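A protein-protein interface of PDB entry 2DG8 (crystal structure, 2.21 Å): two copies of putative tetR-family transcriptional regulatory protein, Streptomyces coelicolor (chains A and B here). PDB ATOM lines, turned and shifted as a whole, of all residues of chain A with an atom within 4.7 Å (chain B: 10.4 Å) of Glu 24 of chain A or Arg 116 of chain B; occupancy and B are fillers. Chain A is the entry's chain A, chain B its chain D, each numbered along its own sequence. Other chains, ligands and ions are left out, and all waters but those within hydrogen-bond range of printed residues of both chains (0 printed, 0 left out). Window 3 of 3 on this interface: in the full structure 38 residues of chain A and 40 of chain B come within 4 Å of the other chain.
Of chain B, only Arg 116 comes within 4 Å of Glu 24 of chain A. Arg 116 of chain B touches just these residues of chain A: Ile 22 (2.8 Å), Ala 23 (2.5 Å), Glu 24 (3.7 Å), Gly 26 (3.2 Å), Gln 101 (3.5 Å), Val 105 (3.4 Å) and Glu 109 (2.6 Å). No residue of chain B comes within 4 Å of Asp 20 of chain A. Of chain B, only Arg 116 comes within 4 Å of Ala 23 of chain A. Glu 25 of chain A touches none of the printed residues of chain B. Printed residues of chain B within 4 Å of Gly 26 of chain A: Arg 116 (3.2 Å). Printed residues of chain A within 4 Å of Thr 112 of chain B: Glu 109 (3.8 Å). Printed residues of chain B within 4 Å of Ile 22 of chain A: Arg 116 (2.8 Å). Pro 118 of chain B touches none of the printed residues of chain A.
O of Ile 22 of chain A sits at hydrogen-bond distance from NH1 of Arg 116 of chain B, at 2.8 Å. O of Ala 23 of chain A sits at hydrogen-bond distance from NH2 of Arg 116 of chain B. NE2 of Gln 101 of chain A lies within hydrogen-bond range of O of Ala 115 of chain B (2.7 Å). The guanidinium group (NH1) of Arg 116 of chain B lies within salt-bridge range of the side-chain carboxylate (OE2) of Glu 109 of chain A (2.6 Å). N of Gly 26 of chain A lies close to NH1 of Arg 116 of chain B (3.4 Å).
The side-chain carboxylate (OE2) of Glu 24 of chain A lies within salt-bridge range of the guanidinium group (NH1) of Arg 38 of chain A, at 3.0 Å. The side-chain hydroxyl (OG1) of Thr 112 of chain B sits at hydrogen-bond distance from the backbone carbonyl oxygen (O) of Gln 108 of chain B, at 3.3 Å. The guanidinium group of Arg 121 of chain B sits at hydrogen-bond distance from the backbone carbonyl oxygen of Ala 114 of chain B (2.8 Å). O of Ala 115 of chain B is in hydrogen-bond range of NH1 of Arg 121 of chain B.
Arg 116 of chain B touches Glu 24 of chain A (NH2 to O, 3.7 Å). Arg 116 of chain B touches Gln 101 of chain A. Gln 101 of chain A touches Arg 121 of chain B (NE2 to NH1, 3.7 Å). Val 105 of chain A touches Arg 116 of chain B (CG1 to CZ, 3.4 Å). Thr 112 of chain B touches Glu 109 of chain A (CG2 to OE2, 3.8 Å).
Hydrophobic or aromatic side chains of chain A that line the printed part of chain B: Val 105. Among the printed residues, 10 pairs touch across the chains.
Position printed for both chains: 109. Of the 10 pairs that touch across the chains among the printed residues, none has its exchanged pair printed and touching as well.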
ATOM      1  N   ASP A  20       2.074 -27.561 -16.263  1.00  0.00           N
ATOM      2  CA  ASP A  20       1.115 -27.353 -15.180  1.00  0.00           C
ATOM      3  C   ASP A  20       0.182 -26.204 -15.578  1.00  0.00           C
ATOM      4  O   ASP A  20      -1.040 -26.327 -15.504  1.00  0.00           O
ATOM      5  CB  ASP A  20       1.833 -26.959 -13.878  1.00  0.00           C
ATOM      6  CG  ASP A  20       2.589 -28.112 -13.236  1.00  0.00           C
ATOM      7  OD1 ASP A  20       3.386 -27.842 -12.309  1.00  0.00           O
ATOM      8  OD2 ASP A  20       2.387 -29.280 -13.639  1.00  0.00           O
ATOM      9  N   LEU A  21       0.778 -25.083 -15.984  1.00  0.00           N
ATOM     10  CA  LEU A  21       0.028 -23.900 -16.389  1.00  0.00           C
ATOM     11  C   LEU A  21      -0.980 -24.203 -17.498  1.00  0.00           C
ATOM     12  O   LEU A  21      -2.156 -23.870 -17.377  1.00  0.00           O
ATOM     13  CB  LEU A  21       1.003 -22.798 -16.839  1.00  0.00           C
ATOM     14  CG  LEU A  21       0.475 -21.415 -17.250  1.00  0.00           C
ATOM     15  CD1 LEU A  21      -0.244 -21.500 -18.590  1.00  0.00           C
ATOM     16  CD2 LEU A  21      -0.461 -20.880 -16.166  1.00  0.00           C
ATOM     17  N   ILE A  22      -0.528 -24.834 -18.577  1.00  0.00           N
ATOM     18  CA  ILE A  22      -1.431 -25.153 -19.682  1.00  0.00           C
ATOM     19  C   ILE A  22      -2.568 -26.064 -19.212  1.00  0.00           C
ATOM     20  O   ILE A  22      -3.740 -25.820 -19.515  1.00  0.00           O
ATOM     21  CB  ILE A  22      -0.666 -25.832 -20.856  1.00  0.00           C
ATOM     22  CG1 ILE A  22       0.316 -24.834 -21.480  1.00  0.00           C
ATOM     23  CG2 ILE A  22      -1.645 -26.327 -21.926  1.00  0.00           C
ATOM     24  CD1 ILE A  22       1.191 -25.436 -22.565  1.00  0.00           C
ATOM     25  N   ALA A  23      -2.224 -27.104 -18.454  1.00  0.00           N
ATOM     26  CA  ALA A  23      -3.230 -28.042 -17.951  1.00  0.00           C
ATOM     27  C   ALA A  23      -4.289 -27.346 -17.090  1.00  0.00           C
ATOM     28  O   ALA A  23      -5.480 -27.584 -17.244  1.00  0.00           O
ATOM     29  CB  ALA A  23      -2.558 -29.143 -17.148  1.00  0.00           C
ATOM     30  N   GLU A  24      -3.845 -26.480 -16.188  1.00  0.00           N
ATOM     31  CA  GLU A  24      -4.748 -25.773 -15.289  1.00  0.00           C
ATOM     32  C   GLU A  24      -5.505 -24.580 -15.864  1.00  0.00           C
ATOM     33  O   GLU A  24      -6.721 -24.484 -15.704  1.00  0.00           O
ATOM     34  CB  GLU A  24      -3.982 -25.311 -14.049  1.00  0.00           C
ATOM     35  CG  GLU A  24      -3.452 -26.437 -13.170  1.00  0.00           C
ATOM     36  CD  GLU A  24      -2.563 -25.927 -12.039  1.00  0.00           C
ATOM     37  OE1 GLU A  24      -2.987 -24.999 -11.311  1.00  0.00           O
ATOM     38  OE2 GLU A  24      -1.445 -26.458 -11.875  1.00  0.00           O
ATOM     39  N   GLU A  25      -4.802 -23.684 -16.549  1.00  0.00           N
ATOM     40  CA  GLU A  25      -5.431 -22.469 -17.075  1.00  0.00           C
ATOM     41  C   GLU A  25      -5.637 -22.397 -18.579  1.00  0.00           C
ATOM     42  O   GLU A  25      -6.319 -21.491 -19.064  1.00  0.00           O
ATOM     43  CB  GLU A  25      -4.620 -21.245 -16.631  1.00  0.00           C
ATOM     44  CG  GLU A  25      -4.541 -21.062 -15.111  1.00  0.00           C
ATOM     45  CD  GLU A  25      -3.618 -19.924 -14.699  1.00  0.00           C
ATOM     46  OE1 GLU A  25      -3.723 -18.830 -15.288  1.00  0.00           O
ATOM     47  OE2 GLU A  25      -2.792 -20.123 -13.783  1.00  0.00           O
ATOM     48  N   GLY A  26      -5.039 -23.327 -19.318  1.00  0.00           N
ATOM     49  CA  GLY A  26      -5.190 -23.316 -20.760  1.00  0.00           C
ATOM     50  C   GLY A  26      -4.020 -22.673 -21.481  1.00  0.00           C
ATOM     51  O   GLY A  26      -3.260 -21.893 -20.896  1.00  0.00           O
ATOM     52  N   ARG A  38       5.526 -20.069 -11.151  1.00  0.00           N
ATOM     53  CA  ARG A  38       5.218 -21.464 -10.846  1.00  0.00           C
ATOM     54  C   ARG A  38       6.492 -22.306 -10.721  1.00  0.00           C
ATOM     55  O   ARG A  38       6.571 -23.215  -9.899  1.00  0.00           O
ATOM     56  CB  ARG A  38       4.326 -22.064 -11.935  1.00  0.00           C
ATOM     57  CG  ARG A  38       2.899 -21.565 -11.948  1.00  0.00           C
ATOM     58  CD  ARG A  38       2.174 -22.105 -13.172  1.00  0.00           C
ATOM     59  NE  ARG A  38       0.737 -21.846 -13.136  1.00  0.00           N
ATOM     60  CZ  ARG A  38      -0.175 -22.735 -12.753  1.00  0.00           C
ATOM     61  NH1 ARG A  38       0.200 -23.951 -12.373  1.00  0.00           N
ATOM     62  NH2 ARG A  38      -1.462 -22.410 -12.754  1.00  0.00           N
ATOM     63  N   GLN A 101      -6.698 -36.726 -15.462  1.00  0.00           N
ATOM     64  CA  GLN A 101      -7.421 -35.680 -16.170  1.00  0.00           C
ATOM     65  C   GLN A 101      -6.415 -34.666 -16.720  1.00  0.00           C
ATOM     66  O   GLN A 101      -6.642 -34.067 -17.769  1.00  0.00           O
ATOM     67  CB  GLN A 101      -8.431 -34.980 -15.246  1.00  0.00           C
ATOM     68  CG  GLN A 101      -9.126 -33.774 -15.886  1.00  0.00           C
ATOM     69  CD  GLN A 101     -10.310 -33.269 -15.079  1.00  0.00           C
ATOM     70  OE1 GLN A 101     -10.260 -33.217 -13.849  1.00  0.00           O
ATOM     71  NE2 GLN A 101     -11.379 -32.880 -15.770  1.00  0.00           N
ATOM     72  N   VAL A 105      -6.289 -33.480 -20.567  1.00  0.00           N
ATOM     73  CA  VAL A 105      -6.349 -32.060 -20.924  1.00  0.00           C
ATOM     74  C   VAL A 105      -5.133 -31.620 -21.754  1.00  0.00           C
ATOM     75  O   VAL A 105      -5.281 -30.908 -22.749  1.00  0.00           O
ATOM     76  CB  VAL A 105      -6.462 -31.174 -19.637  1.00  0.00           C
ATOM     77  CG1 VAL A 105      -6.348 -29.692 -19.985  1.00  0.00           C
ATOM     78  CG2 VAL A 105      -7.787 -31.442 -18.946  1.00  0.00           C
ATOM     79  N   GLU A 109      -5.112 -30.167 -25.427  1.00  0.00           N
ATOM     80  CA  GLU A 109      -4.553 -28.841 -25.697  1.00  0.00           C
ATOM     81  C   GLU A 109      -3.627 -28.970 -26.894  1.00  0.00           C
ATOM     82  O   GLU A 109      -3.702 -28.183 -27.835  1.00  0.00           O
ATOM     83  CB  GLU A 109      -3.763 -28.308 -24.490  1.00  0.00           C
ATOM     84  CG  GLU A 109      -4.624 -27.761 -23.361  1.00  0.00           C
ATOM     85  CD  GLU A 109      -5.252 -26.405 -23.686  1.00  0.00           C
ATOM     86  OE1 GLU A 109      -4.882 -25.800 -24.714  1.00  0.00           O
ATOM     87  OE2 GLU A 109      -6.106 -25.928 -22.904  1.00  0.00           O
ATOM     88  N   ILE B  27     -11.308 -20.649 -27.416  1.00  0.00           N
ATOM     89  CA  ILE B  27     -12.280 -20.709 -26.335  1.00  0.00           C
ATOM     90  C   ILE B  27     -12.079 -19.661 -25.224  1.00  0.00           C
ATOM     91  O   ILE B  27     -13.050 -19.117 -24.692  1.00  0.00           O
ATOM     92  CB  ILE B  27     -12.290 -22.145 -25.726  1.00  0.00           C
ATOM     93  CG1 ILE B  27     -13.424 -22.289 -24.715  1.00  0.00           C
ATOM     94  CG2 ILE B  27     -10.943 -22.459 -25.098  1.00  0.00           C
ATOM     95  CD1 ILE B  27     -14.769 -22.543 -25.362  1.00  0.00           C
ATOM     96  N   ALA B  28     -10.832 -19.361 -24.880  1.00  0.00           N
ATOM     97  CA  ALA B  28     -10.570 -18.384 -23.824  1.00  0.00           C
ATOM     98  C   ALA B  28     -11.042 -16.965 -24.183  1.00  0.00           C
ATOM     99  O   ALA B  28     -11.199 -16.116 -23.308  1.00  0.00           O
ATOM    100  CB  ALA B  28      -9.072 -18.369 -23.475  1.00  0.00           C
ATOM    101  N   LEU B  57     -22.537 -21.931 -24.501  1.00  0.00           N
ATOM    102  CA  LEU B  57     -21.570 -22.828 -25.128  1.00  0.00           C
ATOM    103  C   LEU B  57     -22.259 -24.151 -25.424  1.00  0.00           C
ATOM    104  O   LEU B  57     -22.005 -24.798 -26.437  1.00  0.00           O
ATOM    105  CB  LEU B  57     -20.387 -23.074 -24.189  1.00  0.00           C
ATOM    106  CG  LEU B  57     -19.440 -21.898 -23.968  1.00  0.00           C
ATOM    107  CD1 LEU B  57     -18.370 -22.283 -22.946  1.00  0.00           C
ATOM    108  CD2 LEU B  57     -18.804 -21.513 -25.301  1.00  0.00           C
ATOM    109  N   GLN B 108     -12.022 -29.954 -31.896  1.00  0.00           N
ATOM    110  CA  GLN B 108     -10.956 -29.984 -30.893  1.00  0.00           C
ATOM    111  C   GLN B 108     -11.275 -29.076 -29.713  1.00  0.00           C
ATOM    112  O   GLN B 108     -11.011 -29.432 -28.571  1.00  0.00           O
ATOM    113  CB  GLN B 108      -9.602 -29.601 -31.511  1.00  0.00           C
ATOM    114  CG  GLN B 108      -9.119 -30.560 -32.599  1.00  0.00           C
ATOM    115  CD  GLN B 108      -9.114 -32.023 -32.146  1.00  0.00           C
ATOM    116  OE1 GLN B 108      -8.462 -32.389 -31.164  1.00  0.00           O
ATOM    117  NE2 GLN B 108      -9.847 -32.862 -32.868  1.00  0.00           N
ATOM    118  N   GLU B 109     -11.833 -27.902 -29.981  1.00  0.00           N
ATOM    119  CA  GLU B 109     -12.187 -26.994 -28.895  1.00  0.00           C
ATOM    120  C   GLU B 109     -13.238 -27.673 -27.997  1.00  0.00           C
ATOM    121  O   GLU B 109     -13.152 -27.602 -26.764  1.00  0.00           O
ATOM    122  CB  GLU B 109     -12.723 -25.663 -29.454  1.00  0.00           C
ATOM    123  CG  GLU B 109     -11.638 -24.722 -30.035  1.00  0.00           C
ATOM    124  CD  GLU B 109     -10.828 -23.979 -28.959  1.00  0.00           C
ATOM    125  OE1 GLU B 109      -9.926 -23.188 -29.315  1.00  0.00           O
ATOM    126  OE2 GLU B 109     -11.090 -24.175 -27.758  1.00  0.00           O
ATOM    127  N   LEU B 110     -14.219 -28.338 -28.608  1.00  0.00           N
ATOM    128  CA  LEU B 110     -15.244 -29.033 -27.833  1.00  0.00           C
ATOM    129  C   LEU B 110     -14.603 -30.144 -26.997  1.00  0.00           C
ATOM    130  O   LEU B 110     -14.943 -30.329 -25.832  1.00  0.00           O
ATOM    131  CB  LEU B 110     -16.306 -29.620 -28.763  1.00  0.00           C
ATOM    132  CG  LEU B 110     -17.270 -30.637 -28.142  1.00  0.00           C
ATOM    133  CD1 LEU B 110     -18.017 -30.027 -26.969  1.00  0.00           C
ATOM    134  CD2 LEU B 110     -18.237 -31.102 -29.210  1.00  0.00           C
ATOM    135  N   TYR B 111     -13.666 -30.876 -27.587  1.00  0.00           N
ATOM    136  CA  TYR B 111     -12.995 -31.946 -26.861  1.00  0.00           C
ATOM    137  C   TYR B 111     -12.222 -31.438 -25.642  1.00  0.00           C
ATOM    138  O   TYR B 111     -12.222 -32.073 -24.590  1.00  0.00           O
ATOM    139  CB  TYR B 111     -12.072 -32.729 -27.803  1.00  0.00           C
ATOM    140  CG  TYR B 111     -12.843 -33.602 -28.771  1.00  0.00           C
ATOM    141  CD1 TYR B 111     -14.196 -33.861 -28.563  1.00  0.00           C
ATOM    142  CD2 TYR B 111     -12.231 -34.166 -29.883  1.00  0.00           C
ATOM    143  CE1 TYR B 111     -14.928 -34.657 -29.441  1.00  0.00           C
ATOM    144  CE2 TYR B 111     -12.959 -34.974 -30.774  1.00  0.00           C
ATOM    145  CZ  TYR B 111     -14.310 -35.209 -30.539  1.00  0.00           C
ATOM    146  OH  TYR B 111     -15.063 -35.986 -31.397  1.00  0.00           O
ATOM    147  N   THR B 112     -11.573 -30.287 -25.778  1.00  0.00           N
ATOM    148  CA  THR B 112     -10.825 -29.718 -24.662  1.00  0.00           C
ATOM    149  C   THR B 112     -11.762 -29.262 -23.546  1.00  0.00           C
ATOM    150  O   THR B 112     -11.487 -29.483 -22.366  1.00  0.00           O
ATOM    151  CB  THR B 112      -9.967 -28.531 -25.127  1.00  0.00           C
ATOM    152  OG1 THR B 112      -8.988 -28.995 -26.065  1.00  0.00           O
ATOM    153  CG2 THR B 112      -9.261 -27.875 -23.941  1.00  0.00           C
ATOM    154  N   LEU B 113     -12.872 -28.631 -23.921  1.00  0.00           N
ATOM    155  CA  LEU B 113     -13.847 -28.143 -22.944  1.00  0.00           C
ATOM    156  C   LEU B 113     -14.445 -29.306 -22.156  1.00  0.00           C
ATOM    157  O   LEU B 113     -14.575 -29.235 -20.933  1.00  0.00           O
ATOM    158  CB  LEU B 113     -14.973 -27.364 -23.648  1.00  0.00           C
ATOM    159  CG  LEU B 113     -16.082 -26.791 -22.754  1.00  0.00           C
ATOM    160  CD1 LEU B 113     -15.496 -25.749 -21.810  1.00  0.00           C
ATOM    161  CD2 LEU B 113     -17.178 -26.171 -23.608  1.00  0.00           C
ATOM    162  N   ALA B 114     -14.813 -30.377 -22.853  1.00  0.00           N
ATOM    163  CA  ALA B 114     -15.392 -31.540 -22.187  1.00  0.00           C
ATOM    164  C   ALA B 114     -14.364 -32.242 -21.290  1.00  0.00           C
ATOM    165  O   ALA B 114     -14.716 -32.793 -20.239  1.00  0.00           O
ATOM    166  CB  ALA B 114     -15.960 -32.506 -23.224  1.00  0.00           C
ATOM    167  N   ALA B 115     -13.098 -32.224 -21.693  1.00  0.00           N
ATOM    168  CA  ALA B 115     -12.055 -32.844 -20.874  1.00  0.00           C
ATOM    169  C   ALA B 115     -11.911 -32.071 -19.559  1.00  0.00           C
ATOM    170  O   ALA B 115     -11.772 -32.664 -18.480  1.00  0.00           O
ATOM    171  CB  ALA B 115     -10.715 -32.858 -21.628  1.00  0.00           C
ATOM    172  N   ARG B 116     -11.953 -30.743 -19.663  1.00  0.00           N
ATOM    173  CA  ARG B 116     -11.823 -29.846 -18.507  1.00  0.00           C
ATOM    174  C   ARG B 116     -13.046 -29.782 -17.609  1.00  0.00           C
ATOM    175  O   ARG B 116     -12.915 -29.756 -16.392  1.00  0.00           O
ATOM    176  CB  ARG B 116     -11.546 -28.409 -18.959  1.00  0.00           C
ATOM    177  CG  ARG B 116     -10.148 -28.123 -19.431  1.00  0.00           C
ATOM    178  CD  ARG B 116      -9.985 -26.628 -19.737  1.00  0.00           C
ATOM    179  NE  ARG B 116      -8.695 -26.367 -20.363  1.00  0.00           N
ATOM    180  CZ  ARG B 116      -7.535 -26.474 -19.731  1.00  0.00           C
ATOM    181  NH1 ARG B 116      -6.406 -26.234 -20.378  1.00  0.00           N
ATOM    182  NH2 ARG B 116      -7.512 -26.794 -18.443  1.00  0.00           N
ATOM    183  N   GLN B 117     -14.228 -29.725 -18.217  1.00  0.00           N
ATOM    184  CA  GLN B 117     -15.479 -29.613 -17.474  1.00  0.00           C
ATOM    185  C   GLN B 117     -16.504 -30.701 -17.809  1.00  0.00           C
ATOM    186  O   GLN B 117     -17.317 -30.549 -18.719  1.00  0.00           O
ATOM    187  CB  GLN B 117     -16.082 -28.229 -17.724  1.00  0.00           C
ATOM    188  CG  GLN B 117     -15.143 -27.082 -17.349  1.00  0.00           C
ATOM    189  CD  GLN B 117     -15.676 -25.720 -17.759  1.00  0.00           C
ATOM    190  OE1 GLN B 117     -16.781 -25.331 -17.376  1.00  0.00           O
ATOM    191  NE2 GLN B 117     -14.887 -24.983 -18.540  1.00  0.00           N
ATOM    192  N   PRO B 118     -16.480 -31.810 -17.051  1.00  0.00           N
ATOM    193  CA  PRO B 118     -17.368 -32.963 -17.206  1.00  0.00           C
ATOM    194  C   PRO B 118     -18.807 -32.620 -17.541  1.00  0.00           C
ATOM    195  O   PRO B 118     -19.504 -33.417 -18.158  1.00  0.00           O
ATOM    196  CB  PRO B 118     -17.241 -33.664 -15.862  1.00  0.00           C
ATOM    197  CG  PRO B 118     -15.787 -33.474 -15.550  1.00  0.00           C
ATOM    198  CD  PRO B 118     -15.596 -31.993 -15.884  1.00  0.00           C
ATOM    199  N   ALA B 119     -19.257 -31.439 -17.130  1.00  0.00           N
ATOM    200  CA  ALA B 119     -20.630 -31.027 -17.399  1.00  0.00           C
ATOM    201  C   ALA B 119     -20.895 -31.047 -18.899  1.00  0.00           C
ATOM    202  O   ALA B 119     -21.969 -31.456 -19.353  1.00  0.00           O
ATOM    203  CB  ALA B 119     -20.878 -29.639 -16.848  1.00  0.00           C
ATOM    204  N   TYR B 120     -19.906 -30.610 -19.668  1.00  0.00           N
ATOM    205  CA  TYR B 120     -20.045 -30.580 -21.112  1.00  0.00           C
ATOM    206  C   TYR B 120     -19.970 -31.956 -21.751  1.00  0.00           C
ATOM    207  O   TYR B 120     -20.240 -32.095 -22.944  1.00  0.00           O
ATOM    208  CB  TYR B 120     -18.987 -29.665 -21.727  1.00  0.00           C
ATOM    209  CG  TYR B 120     -19.172 -28.215 -21.349  1.00  0.00           C
ATOM    210  CD1 TYR B 120     -18.426 -27.641 -20.322  1.00  0.00           C
ATOM    211  CD2 TYR B 120     -20.095 -27.415 -22.021  1.00  0.00           C
ATOM    212  CE1 TYR B 120     -18.589 -26.299 -19.976  1.00  0.00           C
ATOM    213  CE2 TYR B 120     -20.272 -26.072 -21.683  1.00  0.00           C
ATOM    214  CZ  TYR B 120     -19.514 -25.521 -20.662  1.00  0.00           C
ATOM    215  OH  TYR B 120     -19.666 -24.191 -20.347  1.00  0.00           O
ATOM    216  N   ARG B 121     -19.621 -32.979 -20.970  1.00  0.00           N
ATOM    217  CA  ARG B 121     -19.539 -34.325 -21.523  1.00  0.00           C
ATOM    218  C   ARG B 121     -20.926 -34.844 -21.868  1.00  0.00           C
ATOM    219  O   ARG B 121     -21.076 -35.934 -22.420  1.00  0.00           O
ATOM    220  CB  ARG B 121     -18.830 -35.272 -20.550  1.00  0.00           C
ATOM    221  CG  ARG B 121     -17.343 -34.978 -20.452  1.00  0.00           C
ATOM    222  CD  ARG B 121     -16.607 -35.866 -19.472  1.00  0.00           C
ATOM    223  NE  ARG B 121     -15.309 -35.275 -19.143  1.00  0.00           N
ATOM    224  CZ  ARG B 121     -14.433 -35.790 -18.286  1.00  0.00           C
ATOM    225  NH1 ARG B 121     -13.286 -35.161 -18.053  1.00  0.00           N
ATOM    226  NH2 ARG B 121     -14.696 -36.936 -17.665  1.00  0.00           N
ATOM    227  N   THR B 124     -21.057 -34.159 -25.670  1.00  0.00           N
ATOM    228  CA  THR B 124     -20.117 -35.009 -26.384  1.00  0.00           C
ATOM    229  C   THR B 124     -20.714 -36.425 -26.328  1.00  0.00           C
ATOM    230  O   THR B 124     -20.572 -37.221 -27.251  1.00  0.00           O
ATOM    231  CB  THR B 124     -18.726 -34.947 -25.734  1.00  0.00           C
ATOM    232  OG1 THR B 124     -17.761 -35.537 -26.611  1.00  0.00           O
ATOM    233  CG2 THR B 124     -18.721 -35.661 -24.427  1.00  0.00           C
